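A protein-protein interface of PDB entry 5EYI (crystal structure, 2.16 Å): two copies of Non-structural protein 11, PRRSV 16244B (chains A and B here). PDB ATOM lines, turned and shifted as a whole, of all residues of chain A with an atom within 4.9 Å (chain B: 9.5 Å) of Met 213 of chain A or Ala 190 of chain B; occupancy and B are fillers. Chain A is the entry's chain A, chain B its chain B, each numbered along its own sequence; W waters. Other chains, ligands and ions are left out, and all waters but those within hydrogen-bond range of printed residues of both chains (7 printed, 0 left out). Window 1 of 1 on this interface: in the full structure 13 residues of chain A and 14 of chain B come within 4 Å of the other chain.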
ATOM      1  N   SER A 198      25.890  -8.115 -16.016  1.00  0.00           N
ATOM      2  CA  SER A 198      26.952  -7.130 -16.195  1.00  0.00           C
ATOM      3  C   SER A 198      27.470  -6.657 -14.850  1.00  0.00           C
ATOM      4  O   SER A 198      26.775  -6.752 -13.848  1.00  0.00           O
ATOM      5  CB  SER A 198      26.474  -5.939 -17.043  1.00  0.00           C
ATOM      6  OG  SER A 198      25.795  -4.967 -16.268  1.00  0.00           O
ATOM      7  N   LYS A 199      28.699  -6.149 -14.842  1.00  0.00           N
ATOM      8  CA  LYS A 199      29.288  -5.565 -13.643  1.00  0.00           C
ATOM      9  C   LYS A 199      30.368  -4.532 -13.969  1.00  0.00           C
ATOM     10  O   LYS A 199      31.113  -4.676 -14.940  1.00  0.00           O
ATOM     11  CB  LYS A 199      29.874  -6.659 -12.754  1.00  0.00           C
ATOM     12  CG  LYS A 199      30.292  -6.147 -11.386  1.00  0.00           C
ATOM     13  CD  LYS A 199      30.481  -7.271 -10.392  1.00  0.00           C
ATOM     14  CE  LYS A 199      30.860  -6.719  -9.025  1.00  0.00           C
ATOM     15  NZ  LYS A 199      30.993  -7.810  -8.013  1.00  0.00           N
ATOM     16  N   CYS A 200      30.441  -3.504 -13.129  1.00  0.00           N
ATOM     17  CA  CYS A 200      31.423  -2.435 -13.243  1.00  0.00           C
ATOM     18  C   CYS A 200      32.390  -2.544 -12.064  1.00  0.00           C
ATOM     19  O   CYS A 200      32.002  -2.283 -10.928  1.00  0.00           O
ATOM     20  CB  CYS A 200      30.722  -1.080 -13.233  1.00  0.00           C
ATOM     21  SG  CYS A 200      31.825   0.354 -13.076  1.00  0.00           S
ATOM     22  N   ARG A 211      37.746   1.850 -14.702  1.00  0.00           N
ATOM     23  CA  ARG A 211      36.649   0.926 -14.501  1.00  0.00           C
ATOM     24  C   ARG A 211      36.737  -0.197 -15.526  1.00  0.00           C
ATOM     25  O   ARG A 211      37.037   0.049 -16.687  1.00  0.00           O
ATOM     26  CB  ARG A 211      35.307   1.653 -14.612  1.00  0.00           C
ATOM     27  CG  ARG A 211      35.105   2.722 -13.543  1.00  0.00           C
ATOM     28  CD  ARG A 211      33.784   3.466 -13.690  1.00  0.00           C
ATOM     29  NE  ARG A 211      33.738   4.664 -12.847  1.00  0.00           N
ATOM     30  CZ  ARG A 211      34.268   5.856 -13.146  1.00  0.00           C
ATOM     31  NH1 ARG A 211      34.912   6.068 -14.295  1.00  0.00           N
ATOM     32  NH2 ARG A 211      34.151   6.860 -12.277  1.00  0.00           N
ATOM     33  N   LEU A 212      36.499  -1.427 -15.088  1.00  0.00           N
ATOM     34  CA  LEU A 212      36.457  -2.581 -15.979  1.00  0.00           C
ATOM     35  C   LEU A 212      35.013  -2.983 -16.068  1.00  0.00           C
ATOM     36  O   LEU A 212      34.401  -3.335 -15.067  1.00  0.00           O
ATOM     37  CB  LEU A 212      37.301  -3.741 -15.438  1.00  0.00           C
ATOM     38  CG  LEU A 212      37.340  -5.033 -16.269  1.00  0.00           C
ATOM     39  CD1 LEU A 212      37.921  -4.808 -17.662  1.00  0.00           C
ATOM     40  CD2 LEU A 212      38.120  -6.103 -15.530  1.00  0.00           C
ATOM     41  N   MET A 213      34.464  -2.909 -17.267  1.00  0.00           N
ATOM     42  CA  MET A 213      33.091  -3.310 -17.507  1.00  0.00           C
ATOM     43  C   MET A 213      33.126  -4.726 -18.013  1.00  0.00           C
ATOM     44  O   MET A 213      33.855  -5.004 -18.959  1.00  0.00           O
ATOM     45  CB  MET A 213      32.445  -2.399 -18.546  1.00  0.00           C
ATOM     46  CG  MET A 213      32.654  -0.917 -18.272  1.00  0.00           C
ATOM     47  SD  MET A 213      32.397  -0.440 -16.553  1.00  0.00           S
ATOM     48  CE  MET A 213      32.127   1.307 -16.805  1.00  0.00           C
ATOM     49  N   VAL A 214      32.365  -5.611 -17.364  1.00  0.00           N
ATOM     50  CA  VAL A 214      32.251  -7.003 -17.782  1.00  0.00           C
ATOM     51  C   VAL A 214      30.784  -7.365 -18.026  1.00  0.00           C
ATOM     52  O   VAL A 214      29.937  -7.128 -17.169  1.00  0.00           O
ATOM     53  CB  VAL A 214      32.841  -7.956 -16.722  1.00  0.00           C
ATOM     54  CG1 VAL A 214      32.666  -9.418 -17.144  1.00  0.00           C
ATOM     55  CG2 VAL A 214      34.312  -7.621 -16.481  1.00  0.00           C
ATOM     56  N   TRP A 215      30.508  -7.930 -19.198  1.00  0.00           N
ATOM     57  CA  TRP A 215      29.250  -8.602 -19.473  1.00  0.00           C
ATOM     58  C   TRP A 215      29.490 -10.108 -19.507  1.00  0.00           C
ATOM     59  O   TRP A 215      30.223 -10.613 -20.373  1.00  0.00           O
ATOM     60  CB  TRP A 215      28.661  -8.140 -20.795  1.00  0.00           C
ATOM     61  CG  TRP A 215      27.953  -6.850 -20.684  1.00  0.00           C
ATOM     62  CD1 TRP A 215      26.617  -6.671 -20.534  1.00  0.00           C
ATOM     63  CD2 TRP A 215      28.536  -5.544 -20.707  1.00  0.00           C
ATOM     64  NE1 TRP A 215      26.319  -5.333 -20.473  1.00  0.00           N
ATOM     65  CE2 TRP A 215      27.480  -4.616 -20.575  1.00  0.00           C
ATOM     66  CE3 TRP A 215      29.847  -5.067 -20.838  1.00  0.00           C
ATOM     67  CZ2 TRP A 215      27.690  -3.237 -20.565  1.00  0.00           C
ATOM     68  CZ3 TRP A 215      30.056  -3.699 -20.822  1.00  0.00           C
ATOM     69  CH2 TRP A 215      28.981  -2.797 -20.687  1.00  0.00           C
ATOM     70  N   THR A 219      31.680  -9.916 -23.038  1.00  0.00           N
ATOM     71  CA  THR A 219      32.742  -8.958 -23.312  1.00  0.00           C
ATOM     72  C   THR A 219      33.214  -8.271 -22.052  1.00  0.00           C
ATOM     73  O   THR A 219      32.586  -8.358 -20.989  1.00  0.00           O
ATOM     74  CB  THR A 219      32.303  -7.920 -24.393  1.00  0.00           C
ATOM     75  OG1 THR A 219      33.451  -7.258 -24.955  1.00  0.00           O
ATOM     76  CG2 THR A 219      31.322  -6.887 -23.822  1.00  0.00           C
ATOM     77  N   ALA A 220      34.349  -7.603 -22.189  1.00  0.00           N
ATOM     78  CA  ALA A 220      34.932  -6.825 -21.114  1.00  0.00           C
ATOM     79  C   ALA A 220      35.859  -5.777 -21.702  1.00  0.00           C
ATOM     80  O   ALA A 220      36.538  -6.025 -22.698  1.00  0.00           O
ATOM     81  CB  ALA A 220      35.686  -7.707 -20.136  1.00  0.00           C
ATOM     82  N   TYR A 221      35.861  -4.606 -21.088  1.00  0.00           N
ATOM     83  CA  TYR A 221      36.710  -3.521 -21.530  1.00  0.00           C
ATOM     84  C   TYR A 221      36.909  -2.527 -20.423  1.00  0.00           C
ATOM     85  O   TYR A 221      36.075  -2.418 -19.510  1.00  0.00           O
ATOM     86  CB  TYR A 221      36.131  -2.821 -22.760  1.00  0.00           C
ATOM     87  CG  TYR A 221      34.745  -2.211 -22.612  1.00  0.00           C
ATOM     88  CD1 TYR A 221      33.638  -2.804 -23.203  1.00  0.00           C
ATOM     89  CD2 TYR A 221      34.551  -1.018 -21.918  1.00  0.00           C
ATOM     90  CE1 TYR A 221      32.375  -2.233 -23.101  1.00  0.00           C
ATOM     91  CE2 TYR A 221      33.300  -0.450 -21.797  1.00  0.00           C
ATOM     92  CZ  TYR A 221      32.210  -1.051 -22.394  1.00  0.00           C
ATOM     93  OH  TYR A 221      30.954  -0.468 -22.281  1.00  0.00           O
ATOM     94  N   GLN A 223      37.688   1.452 -19.073  1.00  0.00           N
ATOM     95  CA  GLN A 223      37.162   2.786 -19.306  1.00  0.00           C
ATOM     96  C   GLN A 223      37.828   3.728 -18.294  1.00  0.00           C
ATOM     97  O   GLN A 223      38.116   3.327 -17.161  1.00  0.00           O
ATOM     98  CB  GLN A 223      35.635   2.709 -19.168  1.00  0.00           C
ATOM     99  CG  GLN A 223      34.870   3.970 -19.483  1.00  0.00           C
ATOM    100  CD  GLN A 223      34.612   4.882 -18.288  1.00  0.00           C
ATOM    101  OE1 GLN A 223      34.106   5.994 -18.442  1.00  0.00           O
ATOM    102  NE2 GLN A 223      34.940   4.418 -17.101  1.00  0.00           N
ATOM    103  N   ARG B 121      25.250  -0.282  -1.871  1.00  0.00           N
ATOM    104  CA  ARG B 121      25.832  -0.389  -3.208  1.00  0.00           C
ATOM    105  C   ARG B 121      25.078   0.503  -4.211  1.00  0.00           C
ATOM    106  O   ARG B 121      25.707   1.248  -4.959  1.00  0.00           O
ATOM    107  CB  ARG B 121      25.845  -1.840  -3.692  1.00  0.00           C
ATOM    108  CG  ARG B 121      26.665  -2.058  -4.956  1.00  0.00           C
ATOM    109  CD  ARG B 121      26.578  -3.489  -5.441  1.00  0.00           C
ATOM    110  NE  ARG B 121      27.183  -3.649  -6.770  1.00  0.00           N
ATOM    111  CZ  ARG B 121      27.084  -4.735  -7.532  1.00  0.00           C
ATOM    112  NH1 ARG B 121      26.398  -5.802  -7.114  1.00  0.00           N
ATOM    113  NH2 ARG B 121      27.659  -4.761  -8.731  1.00  0.00           N
ATOM    114  N   VAL B 125      26.421   3.923  -6.283  1.00  0.00           N
ATOM    115  CA  VAL B 125      26.292   4.101  -7.744  1.00  0.00           C
ATOM    116  C   VAL B 125      25.625   5.442  -8.089  1.00  0.00           C
ATOM    117  O   VAL B 125      26.081   6.149  -8.993  1.00  0.00           O
ATOM    118  CB  VAL B 125      25.513   2.940  -8.414  1.00  0.00           C
ATOM    119  CG1 VAL B 125      25.243   3.237  -9.891  1.00  0.00           C
ATOM    120  CG2 VAL B 125      26.283   1.634  -8.276  1.00  0.00           C
ATOM    121  N   SER B 128      27.984   8.328  -7.501  1.00  0.00           N
ATOM    122  CA  SER B 128      29.023   8.389  -8.535  1.00  0.00           C
ATOM    123  C   SER B 128      28.498   8.879  -9.892  1.00  0.00           C
ATOM    124  O   SER B 128      29.287   9.301 -10.747  1.00  0.00           O
ATOM    125  CB  SER B 128      29.687   7.016  -8.698  1.00  0.00           C
ATOM    126  OG  SER B 128      28.854   6.131  -9.432  1.00  0.00           O
ATOM    127  N   LEU B 129      27.183   8.795 -10.095  1.00  0.00           N
ATOM    128  CA  LEU B 129      26.542   9.204 -11.340  1.00  0.00           C
ATOM    129  C   LEU B 129      25.390  10.184 -11.053  1.00  0.00           C
ATOM    130  O   LEU B 129      24.222   9.827 -11.182  1.00  0.00           O
ATOM    131  CB  LEU B 129      26.043   7.955 -12.069  1.00  0.00           C
ATOM    132  CG  LEU B 129      27.158   7.077 -12.634  1.00  0.00           C
ATOM    133  CD1 LEU B 129      26.696   5.637 -12.799  1.00  0.00           C
ATOM    134  CD2 LEU B 129      27.678   7.647 -13.951  1.00  0.00           C
ATOM    135  N   TYR B 184      17.519  -1.592 -10.368  1.00  0.00           N
ATOM    136  CA  TYR B 184      18.625  -1.602  -9.408  1.00  0.00           C
ATOM    137  C   TYR B 184      19.836  -0.997 -10.141  1.00  0.00           C
ATOM    138  O   TYR B 184      20.238  -1.492 -11.194  1.00  0.00           O
ATOM    139  CB  TYR B 184      18.859  -3.044  -8.939  1.00  0.00           C
ATOM    140  CG  TYR B 184      19.924  -3.246  -7.890  1.00  0.00           C
ATOM    141  CD1 TYR B 184      20.975  -4.136  -8.106  1.00  0.00           C
ATOM    142  CD2 TYR B 184      19.893  -2.558  -6.684  1.00  0.00           C
ATOM    143  CE1 TYR B 184      21.958  -4.341  -7.146  1.00  0.00           C
ATOM    144  CE2 TYR B 184      20.876  -2.750  -5.719  1.00  0.00           C
ATOM    145  CZ  TYR B 184      21.906  -3.651  -5.957  1.00  0.00           C
ATOM    146  OH  TYR B 184      22.896  -3.864  -5.021  1.00  0.00           O
ATOM    147  N   LEU B 185      20.339   0.128  -9.651  1.00  0.00           N
ATOM    148  CA  LEU B 185      21.367   0.884 -10.385  1.00  0.00           C
ATOM    149  C   LEU B 185      22.632   0.077 -10.737  1.00  0.00           C
ATOM    150  O   LEU B 185      23.162   0.239 -11.846  1.00  0.00           O
ATOM    151  CB  LEU B 185      21.741   2.189  -9.672  1.00  0.00           C
ATOM    152  CG  LEU B 185      20.646   3.249  -9.512  1.00  0.00           C
ATOM    153  CD1 LEU B 185      21.201   4.455  -8.765  1.00  0.00           C
ATOM    154  CD2 LEU B 185      20.072   3.684 -10.851  1.00  0.00           C
ATOM    155  N   PRO B 186      23.102  -0.807  -9.832  1.00  0.00           N
ATOM    156  CA  PRO B 186      24.242  -1.663 -10.191  1.00  0.00           C
ATOM    157  C   PRO B 186      24.064  -2.556 -11.415  1.00  0.00           C
ATOM    158  O   PRO B 186      25.072  -2.904 -12.021  1.00  0.00           O
ATOM    159  CB  PRO B 186      24.455  -2.505  -8.931  1.00  0.00           C
ATOM    160  CG  PRO B 186      24.085  -1.566  -7.842  1.00  0.00           C
ATOM    161  CD  PRO B 186      22.861  -0.853  -8.380  1.00  0.00           C
ATOM    162  N   ASP B 187      22.822  -2.913 -11.773  1.00  0.00           N
ATOM    163  CA  ASP B 187      22.526  -3.587 -13.053  1.00  0.00           C
ATOM    164  C   ASP B 187      22.715  -2.694 -14.288  1.00  0.00           C
ATOM    165  O   ASP B 187      22.746  -3.205 -15.411  1.00  0.00           O
ATOM    166  CB  ASP B 187      21.077  -4.088 -13.120  1.00  0.00           C
ATOM    167  CG  ASP B 187      20.772  -5.205 -12.143  1.00  0.00           C
ATOM    168  OD1 ASP B 187      21.689  -5.904 -11.660  1.00  0.00           O
ATOM    169  OD2 ASP B 187      19.569  -5.399 -11.883  1.00  0.00           O
ATOM    170  N   LEU B 188      22.757  -1.377 -14.099  1.00  0.00           N
ATOM    171  CA  LEU B 188      22.960  -0.437 -15.195  1.00  0.00           C
ATOM    172  C   LEU B 188      24.335   0.226 -15.177  1.00  0.00           C
ATOM    173  O   LEU B 188      24.682   0.924 -16.127  1.00  0.00           O
ATOM    174  CB  LEU B 188      21.889   0.659 -15.148  1.00  0.00           C
ATOM    175  CG  LEU B 188      20.440   0.230 -15.355  1.00  0.00           C
ATOM    176  CD1 LEU B 188      19.524   1.439 -15.243  1.00  0.00           C
ATOM    177  CD2 LEU B 188      20.265  -0.454 -16.700  1.00  0.00           C
ATOM    178  N   GLU B 189      25.119  -0.001 -14.124  1.00  0.00           N
ATOM    179  CA  GLU B 189      26.347   0.759 -13.901  1.00  0.00           C
ATOM    180  C   GLU B 189      27.351   0.621 -15.057  1.00  0.00           C
ATOM    181  O   GLU B 189      27.959   1.615 -15.473  1.00  0.00           O
ATOM    182  CB  GLU B 189      26.992   0.335 -12.590  1.00  0.00           C
ATOM    183  CG  GLU B 189      28.084   1.258 -12.088  1.00  0.00           C
ATOM    184  CD  GLU B 189      28.640   0.795 -10.756  1.00  0.00           C
ATOM    185  OE1 GLU B 189      28.377  -0.365 -10.345  1.00  0.00           O
ATOM    186  OE2 GLU B 189      29.334   1.600 -10.104  1.00  0.00           O
ATOM    187  N   ALA B 190      27.487  -0.598 -15.582  1.00  0.00           N
ATOM    188  CA  ALA B 190      28.379  -0.867 -16.714  1.00  0.00           C
ATOM    189  C   ALA B 190      28.043  -0.014 -17.939  1.00  0.00           C
ATOM    190  O   ALA B 190      28.938   0.385 -18.678  1.00  0.00           O
ATOM    191  CB  ALA B 190      28.360  -2.348 -17.077  1.00  0.00           C
ATOM    192  N   TYR B 191      26.758   0.274 -18.125  1.00  0.00           N
ATOM    193  CA  TYR B 191      26.277   1.088 -19.244  1.00  0.00           C
ATOM    194  C   TYR B 191      26.533   2.587 -19.046  1.00  0.00           C
ATOM    195  O   TYR B 191      26.738   3.312 -20.009  1.00  0.00           O
ATOM    196  CB  TYR B 191      24.767   0.882 -19.448  1.00  0.00           C
ATOM    197  CG  TYR B 191      24.361  -0.544 -19.749  1.00  0.00           C
ATOM    198  CD1 TYR B 191      24.242  -0.973 -21.053  1.00  0.00           C
ATOM    199  CD2 TYR B 191      24.095  -1.458 -18.735  1.00  0.00           C
ATOM    200  CE1 TYR B 191      23.877  -2.269 -21.362  1.00  0.00           C
ATOM    201  CE2 TYR B 191      23.732  -2.767 -19.030  1.00  0.00           C
ATOM    202  CZ  TYR B 191      23.619  -3.163 -20.350  1.00  0.00           C
ATOM    203  OH  TYR B 191      23.270  -4.447 -20.682  1.00  0.00           O
ATOM    204  N   LEU B 192      26.503   3.048 -17.802  1.00  0.00           N
ATOM    205  CA  LEU B 192      26.423   4.480 -17.511  1.00  0.00           C
ATOM    206  C   LEU B 192      27.741   5.252 -17.554  1.00  0.00           C
ATOM    207  O   LEU B 192      27.716   6.482 -17.535  1.00  0.00           O
ATOM    208  CB  LEU B 192      25.754   4.683 -16.152  1.00  0.00           C
ATOM    209  CG  LEU B 192      24.324   4.138 -16.093  1.00  0.00           C
ATOM    210  CD1 LEU B 192      23.810   4.148 -14.662  1.00  0.00           C
ATOM    211  CD2 LEU B 192      23.406   4.916 -17.021  1.00  0.00           C
ATOM    212  N   HIS B 193      28.874   4.550 -17.575  1.00  0.00           N
ATOM    213  CA  HIS B 193      30.171   5.193 -17.784  1.00  0.00           C
ATOM    214  C   HIS B 193      30.565   4.904 -19.224  1.00  0.00           C
ATOM    215  O   HIS B 193      30.771   3.738 -19.568  1.00  0.00           O
ATOM    216  CB  HIS B 193      31.229   4.654 -16.831  1.00  0.00           C
ATOM    217  CG  HIS B 193      30.880   4.815 -15.386  1.00  0.00           C
ATOM    218  ND1 HIS B 193      31.173   5.957 -14.670  1.00  0.00           N
ATOM    219  CD2 HIS B 193      30.269   3.976 -14.519  1.00  0.00           C
ATOM    220  CE1 HIS B 193      30.757   5.815 -13.426  1.00  0.00           C
ATOM    221  NE2 HIS B 193      30.201   4.623 -13.309  1.00  0.00           N
ATOM    222  N   PRO B 194      30.641   5.949 -20.079  1.00  0.00           N
ATOM    223  CA  PRO B 194      30.954   5.733 -21.506  1.00  0.00           C
ATOM    224  C   PRO B 194      32.372   5.200 -21.751  1.00  0.00           C
ATOM    225  O   PRO B 194      33.343   5.795 -21.272  1.00  0.00           O
ATOM    226  CB  PRO B 194      30.806   7.130 -22.125  1.00  0.00           C
ATOM    227  CG  PRO B 194      30.918   8.085 -20.991  1.00  0.00           C
ATOM    228  CD  PRO B 194      30.445   7.379 -19.762  1.00  0.00           C
ATOM    229  N   GLU B 195      32.470   4.086 -22.478  1.00  0.00           N
ATOM    230  CA  GLU B 195      33.755   3.565 -22.972  1.00  0.00           C
ATOM    231  C   GLU B 195      34.590   4.653 -23.686  1.00  0.00           C
ATOM    232  O   GLU B 195      35.737   4.914 -23.315  1.00  0.00           O
ATOM    233  CB  GLU B 195      33.507   2.397 -23.938  1.00  0.00           C
ATOM    234  CG  GLU B 195      34.770   1.686 -24.423  1.00  0.00           C
ATOM    235  CD  GLU B 195      34.503   0.691 -25.536  1.00  0.00           C
ATOM    236  OE1 GLU B 195      33.311   0.421 -25.814  1.00  0.00           O
ATOM    237  OE2 GLU B 195      35.492   0.188 -26.124  1.00  0.00           O
ATOM    238  N   THR B 196      34.003   5.263 -24.710  1.00  0.00           N
ATOM    239  CA  THR B 196      34.658   6.344 -25.461  1.00  0.00           C
ATOM    240  C   THR B 196      33.739   7.528 -25.749  1.00  0.00           C
ATOM    241  O   THR B 196      34.120   8.666 -25.509  1.00  0.00           O
ATOM    242  CB  THR B 196      35.238   5.841 -26.799  1.00  0.00           C
ATOM    243  OG1 THR B 196      34.185   5.319 -27.619  1.00  0.00           O
ATOM    244  CG2 THR B 196      36.295   4.760 -26.565  1.00  0.00           C
ATOM    245  N   LYS B 199      26.364   7.181 -26.469  1.00  0.00           N
ATOM    246  CA  LYS B 199      25.879   5.890 -26.965  1.00  0.00           C
ATOM    247  C   LYS B 199      24.431   5.638 -26.569  1.00  0.00           C
ATOM    248  O   LYS B 199      24.015   5.968 -25.456  1.00  0.00           O
ATOM    249  CB  LYS B 199      26.762   4.759 -26.417  1.00  0.00           C
ATOM    250  CG  LYS B 199      26.473   3.370 -26.971  1.00  0.00           C
ATOM    251  CD  LYS B 199      27.597   2.407 -26.611  1.00  0.00           C
ATOM    252  CE  LYS B 199      27.319   0.987 -27.090  1.00  0.00           C
ATOM    253  NZ  LYS B 199      28.524   0.120 -26.929  1.00  0.00           N
ATOM    254  N   TRP B 201      22.169   2.495 -26.062  1.00  0.00           N
ATOM    255  CA  TRP B 201      22.167   1.035 -25.905  1.00  0.00           C
ATOM    256  C   TRP B 201      20.793   0.449 -26.180  1.00  0.00           C
ATOM    257  O   TRP B 201      19.788   1.030 -25.780  1.00  0.00           O
ATOM    258  CB  TRP B 201      22.541   0.644 -24.482  1.00  0.00           C
ATOM    259  CG  TRP B 201      23.897   1.039 -24.048  1.00  0.00           C
ATOM    260  CD1 TRP B 201      24.276   2.241 -23.542  1.00  0.00           C
ATOM    261  CD2 TRP B 201      25.059   0.212 -24.041  1.00  0.00           C
ATOM    262  NE1 TRP B 201      25.611   2.222 -23.226  1.00  0.00           N
ATOM    263  CE2 TRP B 201      26.116   0.982 -23.515  1.00  0.00           C
ATOM    264  CE3 TRP B 201      25.308  -1.119 -24.414  1.00  0.00           C
ATOM    265  CZ2 TRP B 201      27.410   0.477 -23.366  1.00  0.00           C
ATOM    266  CZ3 TRP B 201      26.596  -1.623 -24.265  1.00  0.00           C
ATOM    267  CH2 TRP B 201      27.631  -0.825 -23.745  1.00  0.00           C
ATOM    268  N   MET B 203      18.682  -2.645 -24.952  1.00  0.00           N
ATOM    269  CA  MET B 203      18.689  -3.608 -23.848  1.00  0.00           C
ATOM    270  C   MET B 203      17.286  -4.087 -23.492  1.00  0.00           C
ATOM    271  O   MET B 203      16.290  -3.472 -23.868  1.00  0.00           O
ATOM    272  CB  MET B 203      19.386  -3.010 -22.618  1.00  0.00           C
ATOM    273  CG  MET B 203      18.642  -1.870 -21.934  1.00  0.00           C
ATOM    274  SD  MET B 203      19.472  -1.312 -20.435  1.00  0.00           S
ATOM    275  CE  MET B 203      19.426  -2.792 -19.431  1.00  0.00           C
ATOM    276  N   LEU B 212      18.560   2.804 -23.804  1.00  0.00           N
ATOM    277  CA  LEU B 212      19.237   3.575 -22.770  1.00  0.00           C
ATOM    278  C   LEU B 212      20.246   4.517 -23.436  1.00  0.00           C
ATOM    279  O   LEU B 212      21.219   4.063 -24.042  1.00  0.00           O
ATOM    280  CB  LEU B 212      19.939   2.633 -21.779  1.00  0.00           C
ATOM    281  CG  LEU B 212      20.782   3.277 -20.675  1.00  0.00           C
ATOM    282  CD1 LEU B 212      20.014   4.366 -19.939  1.00  0.00           C
ATOM    283  CD2 LEU B 212      21.283   2.211 -19.706  1.00  0.00           C
ATOM    284  N   VAL B 214      23.152   7.230 -23.137  1.00  0.00           N
ATOM    285  CA  VAL B 214      24.208   7.667 -22.229  1.00  0.00           C
ATOM    286  C   VAL B 214      25.114   8.637 -22.989  1.00  0.00           C
ATOM    287  O   VAL B 214      25.721   8.269 -23.993  1.00  0.00           O
ATOM    288  CB  VAL B 214      25.031   6.467 -21.691  1.00  0.00           C
ATOM    289  CG1 VAL B 214      25.971   6.911 -20.569  1.00  0.00           C
ATOM    290  CG2 VAL B 214      24.100   5.353 -21.217  1.00  0.00           C
ATOM    291  N   LYS B 218      28.087  11.659 -18.989  1.00  0.00           N
ATOM    292  CA  LYS B 218      27.377  10.781 -18.042  1.00  0.00           C
ATOM    293  C   LYS B 218      25.945  11.239 -17.698  1.00  0.00           C
ATOM    294  O   LYS B 218      25.389  10.830 -16.671  1.00  0.00           O
ATOM    295  CB  LYS B 218      28.199  10.541 -16.759  1.00  0.00           C
ATOM    296  CG  LYS B 218      29.630  10.074 -16.990  1.00  0.00           C
ATOM    297  CD  LYS B 218      30.339   9.838 -15.661  1.00  0.00           C
ATOM    298  CE  LYS B 218      31.853   9.958 -15.765  1.00  0.00           C
ATOM    299  NZ  LYS B 218      32.528   8.755 -16.324  1.00  0.00           N
HETATM  300  O   HOH W   1      28.024  -3.004 -11.301  1.00  0.00           O
HETATM  301  O   HOH W   2      31.872   0.349  -9.521  1.00  0.00           O
HETATM  302  O   HOH W   3      30.569   0.801 -24.940  1.00  0.00           O
HETATM  303  O   HOH W   4      26.371  -5.560 -11.306  1.00  0.00           O
HETATM  304  O   HOH W   5      30.379   1.515 -20.707  1.00  0.00           O
HETATM  305  O   HOH W   6      26.401  -2.972 -14.549  1.00  0.00           O
HETATM  306  O   HOH W   7      23.158  -5.738 -16.224  1.00  0.00           O
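N of Trp 201 of chain B is in hydrogen-bond range of O of Leu 212 of chain B (2.7 Å).
The side-chain sulfur of Cys 200 of chain A sits at hydrogen-bond distance from the side-chain sulfur of Met 213 of chain A (3.6 Å).
The backbone NH (N) of Met 213 of chain A lies within hydrogen-bond range of the backbone carbonyl oxygen (O) of Tyr 221 of chain A.
Water W6 lies within hydrogen-bond range of OG of Ser 198 of chain A, N of Ala 190 of chain B, O of Pro 186 of chain B and N of Glu 189 of chain B.
Water W4 lies within hydrogen-bond range of the backbone carbonyl oxygen of Ser 198 of chain A (2.8 Å), the guanidinium group of Arg 121 of chain B (3.0 Å) and the backbone carbonyl oxygen of Pro 186 of chain B (3.0 Å).
Among the printed residues, merely in contact across the chains: Met 213 of chain A with His 193 of chain B, Gln 223 of chain A with His 193 of chain B, Tyr 221 of chain A with Glu 195 of chain B, Ser 198 of chain A with Asp 187 of chain B, Tyr 221 of chain A with Trp 201 of chain B, Trp 215 of chain A with Ala 190 of chain B, Gln 223 of chain A with Glu 195 of chain B, Cys 200 of chain A with Glu 189 of chain B, Ser 198 of chain A with Ala 190 of chain B, Lys 199 of chain A with Arg 121 of chain B, Met 213 of chain A with Ala 190 of chain B, Gln 223 of chain A with Lys 218 of chain B and Trp 215 of chain A with Trp 201 of chain B.
The side-chain hydroxyl of Tyr 191 of chain B sits at hydrogen-bond distance from the indole nitrogen of Trp 215 of chain A.
The side-chain amide oxygen (OE1) of Gln 223 of chain A sits close to the backbone carbonyl oxygen (O) of Pro 194 of chain B (2.9 Å).
ND1 of His 193 of chain B lies close to NE of Arg 211 of chain A, 3.4 Å away.
Of the 23 printed residues of chain B, 10 touch a printed residue of chain A.
Hydrophobic or aromatic side chains of chain B that line the printed part of chain A: Ala 190, Tyr 191, His 193 and Trp 201.
Of the 12 printed residues of chain A, 8 touch a printed residue of chain B.
Hydrophobic or aromatic side chains of chain A within 4 Å of the printed part of chain B: Met 213, Trp 215 and Tyr 221.
Among the printed residues, 16 pairs touch across the chains.
Among the printed residues, no Asp or Glu carboxylate lies within 4 Å of a Lys or Arg side-chain nitrogen of the other chain.
No residue of chain B comes within 4 Å of Leu 212 of chain A.
Printed residues of chain B within 4 Å of Met 213 of chain A: Ala 190 (3.8 Å) and His 193 (3.5 Å).
No residue of chain B comes within 4 Å of Val 214 of chain A.
Of chain B, only Glu 195 (3.6 Å) and Trp 201 (3.6 Å) come within 4 Å of Tyr 221 of chain A.
Of the printed residues of chain A, Asp 187 of chain B touches Ser 198.
Of the printed residues of chain A, His 193 of chain B touches Arg 211, Met 213 and Gln 223.
Of the printed residues of chain A, Pro 194 of chain B touches Gln 223.
Of the printed residues of chain A, Glu 195 of chain B touches Tyr 221 (3.6 Å) and Gln 223 (3.7 Å).
The nearest residue of chain A that does not touch Ala 190 of chain B is Cys 200 of chain A (4.03 Å).
The nearest printed residue of chain A that does not touch Glu 195 of chain B is Met 213 of chain A (6.3 Å).
Positions printed for both chains: 199, 212 and 214.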
